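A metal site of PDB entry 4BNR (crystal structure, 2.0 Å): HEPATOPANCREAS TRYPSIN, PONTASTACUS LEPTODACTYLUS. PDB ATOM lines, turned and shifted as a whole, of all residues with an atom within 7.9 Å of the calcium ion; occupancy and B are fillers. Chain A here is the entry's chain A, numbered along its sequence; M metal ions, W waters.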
ATOM      1  N   THR A 123      13.665 -21.375 -23.091  1.00  0.00           N
ATOM      2  CA  THR A 123      14.244 -22.651 -22.711  1.00  0.00           C
ATOM      3  C   THR A 123      13.261 -23.428 -21.825  1.00  0.00           C
ATOM      4  O   THR A 123      12.971 -23.020 -20.701  1.00  0.00           O
ATOM      5  CB  THR A 123      15.566 -22.461 -21.944  1.00  0.00           C
ATOM      6  OG1 THR A 123      16.471 -21.715 -22.763  1.00  0.00           O
ATOM      7  CG2 THR A 123      16.202 -23.795 -21.585  1.00  0.00           C
ATOM      8  N   VAL A 154      16.533 -33.133 -20.000  1.00  0.00           N
ATOM      9  CA  VAL A 154      17.943 -33.260 -19.664  1.00  0.00           C
ATOM     10  C   VAL A 154      18.671 -32.066 -20.271  1.00  0.00           C
ATOM     11  O   VAL A 154      18.408 -31.702 -21.416  1.00  0.00           O
ATOM     12  CB  VAL A 154      18.529 -34.583 -20.209  1.00  0.00           C
ATOM     13  CG1 VAL A 154      20.035 -34.659 -19.994  1.00  0.00           C
ATOM     14  CG2 VAL A 154      17.854 -35.764 -19.540  1.00  0.00           C
ATOM     15  N   SER A 155      19.549 -31.452 -19.493  1.00  0.00           N
ATOM     16  CA  SER A 155      20.294 -30.292 -19.977  1.00  0.00           C
ATOM     17  C   SER A 155      21.185 -30.656 -21.151  1.00  0.00           C
ATOM     18  O   SER A 155      21.616 -31.806 -21.287  1.00  0.00           O
ATOM     19  CB  SER A 155      21.157 -29.726 -18.848  1.00  0.00           C
ATOM     20  OG  SER A 155      22.177 -30.646 -18.521  1.00  0.00           O
ATOM     21  N   ASP A 156      21.477 -29.657 -21.983  1.00  0.00           N
ATOM     22  CA  ASP A 156      22.339 -29.843 -23.145  1.00  0.00           C
ATOM     23  C   ASP A 156      23.710 -30.400 -22.760  1.00  0.00           C
ATOM     24  O   ASP A 156      24.247 -31.250 -23.464  1.00  0.00           O
ATOM     25  CB  ASP A 156      22.529 -28.521 -23.888  1.00  0.00           C
ATOM     26  CG  ASP A 156      21.366 -28.178 -24.800  1.00  0.00           C
ATOM     27  OD1 ASP A 156      20.285 -28.805 -24.689  1.00  0.00           O
ATOM     28  OD2 ASP A 156      21.522 -27.258 -25.637  1.00  0.00           O
ATOM     29  N   GLU A 157      24.294 -29.927 -21.654  1.00  0.00           N
ATOM     30  CA  GLU A 157      25.621 -30.382 -21.267  1.00  0.00           C
ATOM     31  C   GLU A 157      25.596 -31.824 -20.755  1.00  0.00           C
ATOM     32  O   GLU A 157      26.519 -32.585 -20.998  1.00  0.00           O
ATOM     33  CB  GLU A 157      26.285 -29.435 -20.240  1.00  0.00           C
ATOM     34  CG  GLU A 157      26.041 -29.774 -18.765  1.00  0.00           C
ATOM     35  CD  GLU A 157      27.060 -29.116 -17.839  1.00  0.00           C
ATOM     36  OE1 GLU A 157      27.732 -28.150 -18.269  1.00  0.00           O
ATOM     37  OE2 GLU A 157      27.187 -29.568 -16.675  1.00  0.00           O
ATOM     38  N   ARG A 160      25.123 -33.960 -23.760  1.00  0.00           N
ATOM     39  CA  ARG A 160      26.386 -34.014 -24.479  1.00  0.00           C
ATOM     40  C   ARG A 160      27.361 -34.979 -23.816  1.00  0.00           C
ATOM     41  O   ARG A 160      28.198 -35.588 -24.498  1.00  0.00           O
ATOM     42  CB  ARG A 160      27.008 -32.622 -24.579  1.00  0.00           C
ATOM     43  CG  ARG A 160      26.419 -31.821 -25.701  1.00  0.00           C
ATOM     44  CD  ARG A 160      26.677 -30.330 -25.568  1.00  0.00           C
ATOM     45  NE  ARG A 160      26.098 -29.634 -26.715  1.00  0.00           N
ATOM     46  CZ  ARG A 160      25.725 -28.361 -26.705  1.00  0.00           C
ATOM     47  NH1 ARG A 160      25.867 -27.620 -25.607  1.00  0.00           N
ATOM     48  NH2 ARG A 160      25.205 -27.828 -27.805  1.00  0.00           N
ATOM     49  N   ILE A 168      25.169 -33.380 -30.006  1.00  0.00           N
ATOM     50  CA  ILE A 168      23.967 -32.658 -29.605  1.00  0.00           C
ATOM     51  C   ILE A 168      24.112 -31.188 -29.942  1.00  0.00           C
ATOM     52  O   ILE A 168      24.928 -30.489 -29.354  1.00  0.00           O
ATOM     53  CB  ILE A 168      23.714 -32.794 -28.078  1.00  0.00           C
ATOM     54  CG1 ILE A 168      23.755 -34.266 -27.659  1.00  0.00           C
ATOM     55  CG2 ILE A 168      22.391 -32.157 -27.698  1.00  0.00           C
ATOM     56  CD1 ILE A 168      22.740 -35.144 -28.359  1.00  0.00           C
ATOM     57  N   LEU A 169      23.321 -30.712 -30.914  1.00  0.00           N
ATOM     58  CA  LEU A 169      23.378 -29.311 -31.318  1.00  0.00           C
ATOM     59  C   LEU A 169      22.616 -28.436 -30.325  1.00  0.00           C
ATOM     60  O   LEU A 169      21.763 -28.921 -29.580  1.00  0.00           O
ATOM     61  CB  LEU A 169      22.777 -29.151 -32.716  1.00  0.00           C
ATOM     62  CG  LEU A 169      23.382 -30.022 -33.821  1.00  0.00           C
ATOM     63  CD1 LEU A 169      22.698 -29.731 -35.139  1.00  0.00           C
ATOM     64  CD2 LEU A 169      24.879 -29.796 -33.933  1.00  0.00           C
ATOM     65  N   ASP A 170      22.939 -27.150 -30.311  1.00  0.00           N
ATOM     66  CA  ASP A 170      22.256 -26.188 -29.450  1.00  0.00           C
ATOM     67  C   ASP A 170      20.739 -26.255 -29.644  1.00  0.00           C
ATOM     68  O   ASP A 170      19.977 -26.167 -28.687  1.00  0.00           O
ATOM     69  CB  ASP A 170      22.739 -24.765 -29.740  1.00  0.00           C
ATOM     70  CG  ASP A 170      24.135 -24.479 -29.182  1.00  0.00           C
ATOM     71  OD1 ASP A 170      24.632 -25.283 -28.356  1.00  0.00           O
ATOM     72  OD2 ASP A 170      24.721 -23.443 -29.561  1.00  0.00           O
ATOM     73  N   SER A 171      20.313 -26.457 -30.902  1.00  0.00           N
ATOM     74  CA  SER A 171      18.894 -26.450 -31.255  1.00  0.00           C
ATOM     75  C   SER A 171      18.187 -27.781 -31.010  1.00  0.00           C
ATOM     76  O   SER A 171      17.043 -27.975 -31.445  1.00  0.00           O
ATOM     77  CB  SER A 171      18.739 -26.060 -32.722  1.00  0.00           C
ATOM     78  OG  SER A 171      19.473 -26.940 -33.568  1.00  0.00           O
ATOM     79  N   MET A 172      18.866 -28.692 -30.336  1.00  0.00           N
ATOM     80  CA  MET A 172      18.266 -29.951 -29.920  1.00  0.00           C
ATOM     81  C   MET A 172      18.025 -29.930 -28.413  1.00  0.00           C
ATOM     82  O   MET A 172      18.729 -29.240 -27.691  1.00  0.00           O
ATOM     83  CB  MET A 172      19.187 -31.122 -30.265  1.00  0.00           C
ATOM     84  CG  MET A 172      19.357 -31.340 -31.759  1.00  0.00           C
ATOM     85  SD  MET A 172      20.593 -32.610 -32.099  1.00  0.00           S
ATOM     86  CE  MET A 172      20.537 -32.634 -33.887  1.00  0.00           C
ATOM     87  N   ILE A 173      17.044 -30.702 -27.948  1.00  0.00           N
ATOM     88  CA  ILE A 173      16.766 -30.814 -26.517  1.00  0.00           C
ATOM     89  C   ILE A 173      16.572 -32.282 -26.187  1.00  0.00           C
ATOM     90  O   ILE A 173      16.039 -33.035 -26.994  1.00  0.00           O
ATOM     91  CB  ILE A 173      15.522 -29.989 -26.131  1.00  0.00           C
ATOM     92  CG1 ILE A 173      15.388 -29.882 -24.611  1.00  0.00           C
ATOM     93  CG2 ILE A 173      14.264 -30.581 -26.754  1.00  0.00           C
ATOM     94  CD1 ILE A 173      14.299 -28.927 -24.160  1.00  0.00           C
ATOM     95  N   CYS A 174      17.021 -32.692 -25.005  1.00  0.00           N
ATOM     96  CA  CYS A 174      16.974 -34.093 -24.605  1.00  0.00           C
ATOM     97  C   CYS A 174      16.058 -34.362 -23.422  1.00  0.00           C
ATOM     98  O   CYS A 174      15.861 -33.499 -22.553  1.00  0.00           O
ATOM     99  CB  CYS A 174      18.385 -34.582 -24.272  1.00  0.00           C
ATOM    100  SG  CYS A 174      19.567 -34.291 -25.594  1.00  0.00           S
ATOM    101  N   TYR A 222      15.465 -34.399 -29.253  1.00  0.00           N
ATOM    102  CA  TYR A 222      14.328 -33.743 -29.886  1.00  0.00           C
ATOM    103  C   TYR A 222      14.772 -32.433 -30.544  1.00  0.00           C
ATOM    104  O   TYR A 222      15.723 -31.796 -30.110  1.00  0.00           O
ATOM    105  CB  TYR A 222      13.249 -33.451 -28.842  1.00  0.00           C
ATOM    106  CG  TYR A 222      12.694 -34.681 -28.159  1.00  0.00           C
ATOM    107  CD1 TYR A 222      13.443 -35.366 -27.207  1.00  0.00           C
ATOM    108  CD2 TYR A 222      11.426 -35.161 -28.463  1.00  0.00           C
ATOM    109  CE1 TYR A 222      12.952 -36.507 -26.594  1.00  0.00           C
ATOM    110  CE2 TYR A 222      10.927 -36.302 -27.845  1.00  0.00           C
ATOM    111  CZ  TYR A 222      11.697 -36.971 -26.918  1.00  0.00           C
ATOM    112  OH  TYR A 222      11.195 -38.090 -26.305  1.00  0.00           O
ATOM    113  N   THR A 223      14.078 -32.045 -31.613  1.00  0.00           N
ATOM    114  CA  THR A 223      14.278 -30.733 -32.180  1.00  0.00           C
ATOM    115  C   THR A 223      13.635 -29.747 -31.217  1.00  0.00           C
ATOM    116  O   THR A 223      12.476 -29.897 -30.852  1.00  0.00           O
ATOM    117  CB  THR A 223      13.628 -30.607 -33.565  1.00  0.00           C
ATOM    118  OG1 THR A 223      14.133 -31.643 -34.401  1.00  0.00           O
ATOM    119  CG2 THR A 223      13.930 -29.251 -34.194  1.00  0.00           C
ATOM    120  N   GLU A 224      14.406 -28.762 -30.780  1.00  0.00           N
ATOM    121  CA  GLU A 224      13.910 -27.820 -29.792  1.00  0.00           C
ATOM    122  C   GLU A 224      13.106 -26.743 -30.511  1.00  0.00           C
ATOM    123  O   GLU A 224      13.669 -25.967 -31.275  1.00  0.00           O
ATOM    124  CB  GLU A 224      15.062 -27.211 -29.002  1.00  0.00           C
ATOM    125  CG  GLU A 224      14.630 -26.400 -27.799  1.00  0.00           C
ATOM    126  CD  GLU A 224      15.799 -26.060 -26.890  1.00  0.00           C
ATOM    127  OE1 GLU A 224      16.950 -26.303 -27.296  1.00  0.00           O
ATOM    128  OE2 GLU A 224      15.561 -25.546 -25.772  1.00  0.00           O
ATOM    129  N   SER A 226      11.586 -23.966 -29.670  1.00  0.00           N
ATOM    130  CA  SER A 226      11.821 -22.553 -29.383  1.00  0.00           C
ATOM    131  C   SER A 226      12.872 -21.919 -30.289  1.00  0.00           C
ATOM    132  O   SER A 226      12.940 -20.707 -30.427  1.00  0.00           O
ATOM    133  CB  SER A 226      12.240 -22.357 -27.916  1.00  0.00           C
ATOM    134  OG  SER A 226      13.575 -22.788 -27.713  1.00  0.00           O
ATOM    135  N   TYR A 227      13.712 -22.748 -30.902  1.00  0.00           N
ATOM    136  CA  TYR A 227      14.708 -22.257 -31.854  1.00  0.00           C
ATOM    137  C   TYR A 227      14.076 -21.944 -33.202  1.00  0.00           C
ATOM    138  O   TYR A 227      14.666 -21.223 -34.002  1.00  0.00           O
ATOM    139  CB  TYR A 227      15.819 -23.295 -32.039  1.00  0.00           C
ATOM    140  CG  TYR A 227      16.924 -23.191 -31.014  1.00  0.00           C
ATOM    141  CD1 TYR A 227      16.735 -23.651 -29.701  1.00  0.00           C
ATOM    142  CD2 TYR A 227      18.148 -22.636 -31.332  1.00  0.00           C
ATOM    143  CE1 TYR A 227      17.744 -23.550 -28.755  1.00  0.00           C
ATOM    144  CE2 TYR A 227      19.163 -22.526 -30.397  1.00  0.00           C
ATOM    145  CZ  TYR A 227      18.949 -22.990 -29.111  1.00  0.00           C
ATOM    146  OH  TYR A 227      19.955 -22.895 -28.172  1.00  0.00           O
HETATM  147 CA    CA M   1      19.102 -27.141 -26.470  1.00  0.00          CA
HETATM  148  O   HOH W   1      19.249 -24.592 -25.830  1.00  0.00           O
HETATM  149  O   HOH W   2      17.755 -26.996 -24.513  1.00  0.00           O
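The calcium ion is bound by water W2, OE1 of Glu 224, O of Met 172, OD2 of Asp 156, O of Asp 170, water W1 and OD1 of Asp 156.
The backbone NH (N) of Leu 169 lies within hydrogen-bond range of the side-chain sulfur (SD) of Met 172 (3.5 Å). OH of Tyr 227 lies close to O of Asp 170. The side-chain carboxylate (OD1) of Asp 170 is in salt-bridge range of the guanidinium group (NH2) of Arg 160. The backbone NH (N) of Glu 224 sits at hydrogen-bond distance from the backbone carbonyl oxygen (O) of Ser 171 (2.8 Å).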
